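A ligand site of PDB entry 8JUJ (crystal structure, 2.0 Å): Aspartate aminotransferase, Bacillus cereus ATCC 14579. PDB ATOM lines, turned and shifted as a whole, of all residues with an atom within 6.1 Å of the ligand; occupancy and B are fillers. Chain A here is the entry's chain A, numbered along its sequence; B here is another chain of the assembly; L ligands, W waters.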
ATOM      1  N   ALA A  32      11.170 -20.974 -16.756  1.00  0.00           N
ATOM      2  CA  ALA A  32      12.083 -21.048 -17.910  1.00  0.00           C
ATOM      3  C   ALA A  32      11.554 -20.215 -19.095  1.00  0.00           C
ATOM      4  O   ALA A  32      12.295 -20.089 -20.069  1.00  0.00           O
ATOM      5  CB  ALA A  32      12.262 -22.488 -18.314  1.00  0.00           C
ATOM      6  N   ALA A  89       9.252 -32.864 -30.992  1.00  0.00           N
ATOM      7  CA  ALA A  89       8.293 -32.277 -30.021  1.00  0.00           C
ATOM      8  C   ALA A  89       9.070 -31.832 -28.787  1.00  0.00           C
ATOM      9  O   ALA A  89       8.822 -32.417 -27.734  1.00  0.00           O
ATOM     10  CB  ALA A  89       7.214 -33.281 -29.646  1.00  0.00           C
ATOM     11  N   GLY A  90      10.009 -30.881 -28.950  1.00  0.00           N
ATOM     12  CA  GLY A  90      10.918 -30.396 -27.889  1.00  0.00           C
ATOM     13  C   GLY A  90      12.376 -30.705 -28.194  1.00  0.00           C
ATOM     14  O   GLY A  90      12.666 -31.636 -28.982  1.00  0.00           O
ATOM     15  N   ILE A  91      13.279 -29.987 -27.508  1.00  0.00           N
ATOM     16  CA  ILE A  91      14.761 -30.043 -27.676  1.00  0.00           C
ATOM     17  C   ILE A  91      15.327 -31.096 -26.731  1.00  0.00           C
ATOM     18  O   ILE A  91      16.327 -31.727 -27.075  1.00  0.00           O
ATOM     19  CB  ILE A  91      15.382 -28.655 -27.445  1.00  0.00           C
ATOM     20  CG1 ILE A  91      14.779 -27.624 -28.415  1.00  0.00           C
ATOM     21  CG2 ILE A  91      16.910 -28.699 -27.500  1.00  0.00           C
ATOM     22  CD1 ILE A  91      15.221 -27.779 -29.858  1.00  0.00           C
ATOM     23  N   VAL A  92      14.760 -31.269 -25.552  1.00  0.00           N
ATOM     24  CA  VAL A  92      15.265 -32.359 -24.674  1.00  0.00           C
ATOM     25  C   VAL A  92      15.051 -33.715 -25.367  1.00  0.00           C
ATOM     26  O   VAL A  92      15.978 -34.531 -25.359  1.00  0.00           O
ATOM     27  CB  VAL A  92      14.701 -32.258 -23.247  1.00  0.00           C
ATOM     28  CG1 VAL A  92      15.175 -33.412 -22.385  1.00  0.00           C
ATOM     29  CG2 VAL A  92      15.103 -30.925 -22.629  1.00  0.00           C
ATOM     30  N   PRO A  93      13.908 -34.024 -26.026  1.00  0.00           N
ATOM     31  CA  PRO A  93      13.787 -35.240 -26.844  1.00  0.00           C
ATOM     32  C   PRO A  93      14.830 -35.379 -27.959  1.00  0.00           C
ATOM     33  O   PRO A  93      15.413 -36.459 -28.116  1.00  0.00           O
ATOM     34  CB  PRO A  93      12.361 -35.188 -27.390  1.00  0.00           C
ATOM     35  CG  PRO A  93      11.631 -34.384 -26.352  1.00  0.00           C
ATOM     36  CD  PRO A  93      12.625 -33.308 -25.975  1.00  0.00           C
ATOM     37  N   LEU A  95      17.854 -34.094 -27.854  1.00  0.00           N
ATOM     38  CA  LEU A  95      19.121 -34.406 -27.153  1.00  0.00           C
ATOM     39  C   LEU A  95      19.205 -35.914 -26.915  1.00  0.00           C
ATOM     40  O   LEU A  95      20.241 -36.534 -27.214  1.00  0.00           O
ATOM     41  CB  LEU A  95      19.196 -33.641 -25.827  1.00  0.00           C
ATOM     42  CG  LEU A  95      19.182 -32.118 -25.922  1.00  0.00           C
ATOM     43  CD1 LEU A  95      19.059 -31.496 -24.540  1.00  0.00           C
ATOM     44  CD2 LEU A  95      20.399 -31.572 -26.640  1.00  0.00           C
ATOM     45  N   ILE A 115      25.578 -25.881 -16.686  1.00  0.00           N
ATOM     46  CA  ILE A 115      24.740 -26.183 -17.876  1.00  0.00           C
ATOM     47  C   ILE A 115      23.354 -26.672 -17.424  1.00  0.00           C
ATOM     48  O   ILE A 115      23.245 -27.332 -16.372  1.00  0.00           O
ATOM     49  CB  ILE A 115      25.489 -27.170 -18.795  1.00  0.00           C
ATOM     50  CG1 ILE A 115      24.743 -27.446 -20.100  1.00  0.00           C
ATOM     51  CG2 ILE A 115      25.795 -28.457 -18.057  1.00  0.00           C
ATOM     52  CD1 ILE A 115      24.459 -26.221 -20.899  1.00  0.00           C
ATOM     53  N   TYR A 116      22.356 -26.306 -18.208  1.00  0.00           N
ATOM     54  CA  TYR A 116      20.953 -26.785 -18.154  1.00  0.00           C
ATOM     55  C   TYR A 116      20.902 -28.244 -17.737  1.00  0.00           C
ATOM     56  O   TYR A 116      21.418 -29.115 -18.419  1.00  0.00           O
ATOM     57  CB  TYR A 116      20.297 -26.590 -19.525  1.00  0.00           C
ATOM     58  CG  TYR A 116      18.804 -26.820 -19.566  1.00  0.00           C
ATOM     59  CD1 TYR A 116      17.963 -26.284 -18.601  1.00  0.00           C
ATOM     60  CD2 TYR A 116      18.233 -27.533 -20.603  1.00  0.00           C
ATOM     61  CE1 TYR A 116      16.587 -26.486 -18.642  1.00  0.00           C
ATOM     62  CE2 TYR A 116      16.856 -27.738 -20.666  1.00  0.00           C
ATOM     63  CZ  TYR A 116      16.033 -27.204 -19.684  1.00  0.00           C
ATOM     64  OH  TYR A 116      14.672 -27.412 -19.752  1.00  0.00           O
ATOM     65  N   PHE A 119      20.778 -31.592 -19.879  1.00  0.00           N
ATOM     66  CA  PHE A 119      22.060 -31.982 -20.539  1.00  0.00           C
ATOM     67  C   PHE A 119      22.650 -33.224 -19.815  1.00  0.00           C
ATOM     68  O   PHE A 119      22.999 -34.225 -20.471  1.00  0.00           O
ATOM     69  CB  PHE A 119      23.071 -30.837 -20.607  1.00  0.00           C
ATOM     70  CG  PHE A 119      22.950 -29.964 -21.838  1.00  0.00           C
ATOM     71  CD1 PHE A 119      21.728 -29.426 -22.206  1.00  0.00           C
ATOM     72  CD2 PHE A 119      24.048 -29.739 -22.657  1.00  0.00           C
ATOM     73  CE1 PHE A 119      21.607 -28.658 -23.350  1.00  0.00           C
ATOM     74  CE2 PHE A 119      23.923 -28.963 -23.802  1.00  0.00           C
ATOM     75  CZ  PHE A 119      22.707 -28.431 -24.148  1.00  0.00           C
ATOM     76  N   CYS A 163      25.778 -25.811 -25.983  1.00  0.00           N
ATOM     77  CA  CYS A 163      24.615 -24.934 -25.727  1.00  0.00           C
ATOM     78  C   CYS A 163      25.042 -23.556 -26.212  1.00  0.00           C
ATOM     79  O   CYS A 163      25.992 -22.994 -25.641  1.00  0.00           O
ATOM     80  CB  CYS A 163      24.196 -24.968 -24.261  1.00  0.00           C
ATOM     81  SG  CYS A 163      22.558 -24.243 -23.940  1.00  0.00           S
ATOM     82  N   PRO A 165      23.080 -19.923 -27.833  1.00  0.00           N
ATOM     83  CA  PRO A 165      23.664 -19.388 -26.606  1.00  0.00           C
ATOM     84  C   PRO A 165      23.554 -20.313 -25.364  1.00  0.00           C
ATOM     85  O   PRO A 165      22.588 -21.093 -25.281  1.00  0.00           O
ATOM     86  CB  PRO A 165      22.807 -18.165 -26.298  1.00  0.00           C
ATOM     87  CG  PRO A 165      22.151 -17.795 -27.610  1.00  0.00           C
ATOM     88  CD  PRO A 165      22.016 -19.082 -28.386  1.00  0.00           C
ATOM     89  N   ASN A 167      22.816 -21.561 -21.809  1.00  0.00           N
ATOM     90  CA  ASN A 167      21.978 -21.463 -20.574  1.00  0.00           C
ATOM     91  C   ASN A 167      22.730 -22.139 -19.435  1.00  0.00           C
ATOM     92  O   ASN A 167      23.038 -23.337 -19.560  1.00  0.00           O
ATOM     93  CB  ASN A 167      20.613 -22.108 -20.808  1.00  0.00           C
ATOM     94  CG  ASN A 167      19.754 -22.303 -19.563  1.00  0.00           C
ATOM     95  OD1 ASN A 167      20.131 -21.944 -18.454  1.00  0.00           O
ATOM     96  ND2 ASN A 167      18.590 -22.884 -19.754  1.00  0.00           N
ATOM     97  N   ASP A 195      22.559 -27.204 -29.257  1.00  0.00           N
ATOM     98  CA  ASP A 195      21.281 -26.732 -28.694  1.00  0.00           C
ATOM     99  C   ASP A 195      21.237 -25.211 -28.896  1.00  0.00           C
ATOM    100  O   ASP A 195      21.772 -24.444 -28.057  1.00  0.00           O
ATOM    101  CB  ASP A 195      21.127 -27.126 -27.231  1.00  0.00           C
ATOM    102  CG  ASP A 195      19.791 -26.713 -26.620  1.00  0.00           C
ATOM    103  OD1 ASP A 195      19.178 -25.735 -27.130  1.00  0.00           O
ATOM    104  OD2 ASP A 195      19.343 -27.412 -25.668  1.00  0.00           O
ATOM    105  N   ILE A 197      18.379 -23.307 -29.121  1.00  0.00           N
ATOM    106  CA  ILE A 197      16.988 -22.891 -28.772  1.00  0.00           C
ATOM    107  C   ILE A 197      16.956 -21.382 -28.439  1.00  0.00           C
ATOM    108  O   ILE A 197      15.892 -20.791 -28.642  1.00  0.00           O
ATOM    109  CB  ILE A 197      16.373 -23.740 -27.648  1.00  0.00           C
ATOM    110  CG1 ILE A 197      14.847 -23.630 -27.628  1.00  0.00           C
ATOM    111  CG2 ILE A 197      16.961 -23.416 -26.288  1.00  0.00           C
ATOM    112  CD1 ILE A 197      14.181 -24.354 -26.457  1.00  0.00           C
ATOM    113  N   HIS A 198      18.024 -20.784 -27.908  1.00  0.00           N
ATOM    114  CA  HIS A 198      18.004 -19.349 -27.471  1.00  0.00           C
ATOM    115  C   HIS A 198      18.551 -18.433 -28.582  1.00  0.00           C
ATOM    116  O   HIS A 198      18.868 -17.284 -28.254  1.00  0.00           O
ATOM    117  CB  HIS A 198      18.773 -19.172 -26.146  1.00  0.00           C
ATOM    118  CG  HIS A 198      18.193 -19.884 -24.965  1.00  0.00           C
ATOM    119  ND1 HIS A 198      17.213 -19.325 -24.174  1.00  0.00           N
ATOM    120  CD2 HIS A 198      18.437 -21.100 -24.444  1.00  0.00           C
ATOM    121  CE1 HIS A 198      16.900 -20.154 -23.197  1.00  0.00           C
ATOM    122  NE2 HIS A 198      17.587 -21.260 -23.363  1.00  0.00           N
ATOM    123  N   ALA A 227      14.073 -23.847 -32.210  1.00  0.00           N
ATOM    124  CA  ALA A 227      12.618 -23.815 -31.982  1.00  0.00           C
ATOM    125  C   ALA A 227      12.121 -22.395 -31.819  1.00  0.00           C
ATOM    126  O   ALA A 227      12.858 -21.517 -31.400  1.00  0.00           O
ATOM    127  CB  ALA A 227      12.281 -24.658 -30.770  1.00  0.00           C
ATOM    128  N   SER A 229       9.867 -21.891 -29.607  1.00  0.00           N
ATOM    129  CA  SER A 229       9.361 -22.103 -28.218  1.00  0.00           C
ATOM    130  C   SER A 229       9.720 -20.956 -27.291  1.00  0.00           C
ATOM    131  O   SER A 229       8.795 -20.303 -26.771  1.00  0.00           O
ATOM    132  CB  SER A 229       9.854 -23.448 -27.686  1.00  0.00           C
ATOM    133  OG  SER A 229       9.588 -24.459 -28.642  1.00  0.00           O
ATOM    134  N   LYS A 230      11.002 -20.717 -27.068  1.00  0.00           N
ATOM    135  CA  LYS A 230      11.505 -19.695 -26.112  1.00  0.00           C
ATOM    136  C   LYS A 230      11.269 -18.287 -26.678  1.00  0.00           C
ATOM    137  O   LYS A 230      10.763 -17.426 -25.918  1.00  0.00           O
ATOM    138  CB  LYS A 230      12.995 -19.909 -25.835  1.00  0.00           C
ATOM    139  CG  LYS A 230      13.336 -21.258 -25.217  1.00  0.00           C
ATOM    140  CD  LYS A 230      13.248 -21.285 -23.709  1.00  0.00           C
ATOM    141  CE  LYS A 230      12.103 -22.118 -23.193  1.00  0.00           C
ATOM    142  NZ  LYS A 230      11.997 -21.999 -21.721  1.00  0.00           N
ATOM    143  N   ALA A 235       6.433 -22.563 -26.007  1.00  0.00           N
ATOM    144  CA  ALA A 235       7.014 -23.860 -25.577  1.00  0.00           C
ATOM    145  C   ALA A 235       5.900 -24.896 -25.344  1.00  0.00           C
ATOM    146  O   ALA A 235       6.141 -26.072 -25.575  1.00  0.00           O
ATOM    147  CB  ALA A 235       7.833 -23.666 -24.340  1.00  0.00           C
ATOM    148  N   ALA A 239       6.776 -27.226 -30.609  1.00  0.00           N
ATOM    149  CA  ALA A 239       7.334 -27.188 -31.973  1.00  0.00           C
ATOM    150  C   ALA A 239       8.852 -27.030 -31.865  1.00  0.00           C
ATOM    151  O   ALA A 239       9.273 -26.080 -31.210  1.00  0.00           O
ATOM    152  CB  ALA A 239       6.697 -26.066 -32.745  1.00  0.00           C
ATOM    153  N   SER A 240       9.619 -27.944 -32.474  1.00  0.00           N
ATOM    154  CA  SER A 240      11.095 -27.819 -32.608  1.00  0.00           C
ATOM    155  C   SER A 240      11.491 -28.276 -33.997  1.00  0.00           C
ATOM    156  O   SER A 240      10.817 -29.168 -34.555  1.00  0.00           O
ATOM    157  CB  SER A 240      11.853 -28.615 -31.563  1.00  0.00           C
ATOM    158  OG  SER A 240      11.292 -28.468 -30.268  1.00  0.00           O
ATOM    159  N   LEU A 319      17.768 -14.847 -19.190  1.00  0.00           N
ATOM    160  CA  LEU A 319      18.203 -15.461 -17.923  1.00  0.00           C
ATOM    161  C   LEU A 319      19.394 -14.662 -17.374  1.00  0.00           C
ATOM    162  O   LEU A 319      20.229 -14.257 -18.185  1.00  0.00           O
ATOM    163  CB  LEU A 319      18.606 -16.909 -18.207  1.00  0.00           C
ATOM    164  CG  LEU A 319      17.556 -17.712 -18.983  1.00  0.00           C
ATOM    165  CD1 LEU A 319      18.060 -19.128 -19.260  1.00  0.00           C
ATOM    166  CD2 LEU A 319      16.232 -17.734 -18.246  1.00  0.00           C
ATOM    167  N   ARG A 361      19.808 -18.424 -10.736  1.00  0.00           N
ATOM    168  CA  ARG A 361      19.354 -17.889 -12.027  1.00  0.00           C
ATOM    169  C   ARG A 361      17.970 -17.269 -11.829  1.00  0.00           C
ATOM    170  O   ARG A 361      17.125 -17.832 -11.078  1.00  0.00           O
ATOM    171  CB  ARG A 361      19.385 -18.992 -13.080  1.00  0.00           C
ATOM    172  CG  ARG A 361      19.237 -18.492 -14.512  1.00  0.00           C
ATOM    173  CD  ARG A 361      18.295 -19.418 -15.261  1.00  0.00           C
ATOM    174  NE  ARG A 361      16.967 -19.114 -14.763  1.00  0.00           N
ATOM    175  CZ  ARG A 361      15.855 -19.814 -14.946  1.00  0.00           C
ATOM    176  NH1 ARG A 361      14.729 -19.336 -14.436  1.00  0.00           N
ATOM    177  NH2 ARG A 361      15.841 -20.931 -15.654  1.00  0.00           N
ATOM    178  N   TYR B  57       5.089 -23.568 -20.846  1.00  0.00           N
ATOM    179  CA  TYR B  57       5.038 -24.931 -20.260  1.00  0.00           C
ATOM    180  C   TYR B  57       3.847 -24.954 -19.307  1.00  0.00           C
ATOM    181  O   TYR B  57       3.639 -23.994 -18.551  1.00  0.00           O
ATOM    182  CB  TYR B  57       6.340 -25.303 -19.530  1.00  0.00           C
ATOM    183  CG  TYR B  57       7.560 -25.338 -20.415  1.00  0.00           C
ATOM    184  CD1 TYR B  57       7.723 -26.300 -21.420  1.00  0.00           C
ATOM    185  CD2 TYR B  57       8.588 -24.401 -20.261  1.00  0.00           C
ATOM    186  CE1 TYR B  57       8.840 -26.303 -22.242  1.00  0.00           C
ATOM    187  CE2 TYR B  57       9.702 -24.405 -21.074  1.00  0.00           C
ATOM    188  CZ  TYR B  57       9.844 -25.355 -22.075  1.00  0.00           C
ATOM    189  OH  TYR B  57      10.954 -25.325 -22.864  1.00  0.00           O
ATOM    190  N   GLY B 261      13.072 -37.957 -23.016  1.00  0.00           N
ATOM    191  CA  GLY B 261      12.907 -36.494 -22.925  1.00  0.00           C
ATOM    192  C   GLY B 261      11.454 -36.065 -22.927  1.00  0.00           C
ATOM    193  O   GLY B 261      11.205 -34.877 -23.122  1.00  0.00           O
ATOM    194  N   HIS B 263       8.049 -34.783 -21.452  1.00  0.00           N
ATOM    195  CA  HIS B 263       7.604 -34.009 -20.264  1.00  0.00           C
ATOM    196  C   HIS B 263       6.199 -33.432 -20.534  1.00  0.00           C
ATOM    197  O   HIS B 263       6.035 -32.193 -20.525  1.00  0.00           O
ATOM    198  CB  HIS B 263       8.692 -32.983 -19.869  1.00  0.00           C
ATOM    199  CG  HIS B 263       9.421 -32.338 -21.025  1.00  0.00           C
ATOM    200  ND1 HIS B 263       8.767 -31.907 -22.183  1.00  0.00           N
ATOM    201  CD2 HIS B 263      10.733 -32.043 -21.201  1.00  0.00           C
ATOM    202  CE1 HIS B 263       9.648 -31.390 -23.021  1.00  0.00           C
ATOM    203  NE2 HIS B 263      10.864 -31.446 -22.431  1.00  0.00           N
HETATM  204  N1  LIG L   1      17.458 -26.314 -24.125  1.00  0.00           N
HETATM  205  C1  LIG L   1      17.810 -25.206 -23.459  1.00  0.00           C
HETATM  206  C2  LIG L   1      19.213 -24.720 -23.554  1.00  0.00           C
HETATM  207  C3  LIG L   1      16.857 -24.513 -22.711  1.00  0.00           C
HETATM  208  O1  LIG L   1      17.199 -23.420 -22.029  1.00  0.00           O
HETATM  209  C4  LIG L   1      15.537 -24.980 -22.638  1.00  0.00           C
HETATM  210  C5  LIG L   1      14.591 -24.262 -21.790  1.00  0.00           C
HETATM  211  O2  LIG L   1      14.794 -23.955 -20.630  1.00  0.00           O
HETATM  212  C6  LIG L   1      15.195 -26.153 -23.328  1.00  0.00           C
HETATM  213  C7  LIG L   1      16.178 -26.762 -24.058  1.00  0.00           C
HETATM  214  C8  LIG L   1      13.794 -26.677 -23.278  1.00  0.00           C
HETATM  215  O3  LIG L   1      13.599 -27.855 -24.118  1.00  0.00           O
HETATM  216  P1  LIG L   1      12.125 -28.371 -24.656  1.00  0.00           P
HETATM  217  O4  LIG L   1      12.205 -29.935 -24.637  1.00  0.00           O
HETATM  218  O5  LIG L   1      11.091 -27.810 -23.671  1.00  0.00           O
HETATM  219  O6  LIG L   1      12.005 -27.754 -26.079  1.00  0.00           O
HETATM  220  O   HOH W   1      14.547 -20.831 -20.475  1.00  0.00           O
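Water W1 lies within hydrogen-bond range of the backbone carbonyl oxygen (O) of Ala 32 (2.4 Å), the side-chain amino group (NZ) of Lys 230 (3.1 Å) and an oxygen (O2) of the ligand (3.1 Å).
Ala 32 touches the ligand (CB to O2, 3.7 Å). Gly 90 touches the ligand. Pro 93 touches the ligand (CD to O4, 3.7 Å). Tyr 116 touches the ligand. Cys 163 touches the ligand. Ile 197 touches the ligand (CG2 to C1, 3.5 Å). Lys 230 touches the ligand. The nearest printed residue that does not touch the ligand is Ser 240 (4.3 Å).
N of Ile 197 is in hydrogen-bond range of OD1 of Asp 195. The backbone NH (N) of Asn 167 lies within hydrogen-bond range of the side-chain sulfur (SG) of Cys 163 (3.4 Å). N of Tyr 116 sits at hydrogen-bond distance from O of Asn 167, 3.3 Å away. The side-chain hydroxyl of Ser 240 lies within hydrogen-bond range of the backbone NH of Gly 90, at 3.0 Å. The side-chain sulfur (SG) of Cys 163 sits at hydrogen-bond distance from the backbone carbonyl oxygen (O) of Pro 165 (3.4 Å). The backbone carbonyl oxygen (O) of Ala 32 sits at hydrogen-bond distance from the side-chain amino group (NZ) of Lys 230.
A ring nitrogen (NE2) of His 198 is in hydrogen-bond range of an oxygen (O1) of the ligand (2.6 Å). The side-chain hydroxyl (OH) of Tyr 57 of chain B sits at hydrogen-bond distance from an oxygen (O5) of the ligand (2.6 Å). N1 of the ligand is in hydrogen-bond range of OD2 of Asp 195, at 2.7 Å. An oxygen (O1) of the ligand sits at hydrogen-bond distance from the side-chain amide nitrogen (ND2) of Asn 167 (2.7 Å). The backbone NH (N) of Ile 91 is in hydrogen-bond range of an oxygen (O6) of the ligand. An oxygen (O4) of the ligand sits at hydrogen-bond distance from a ring nitrogen (NE2) of His 263 of chain B, 3.0 Å away. The backbone NH (N) of Val 92 lies within hydrogen-bond range of an oxygen (O4) of the ligand (3.0 Å).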
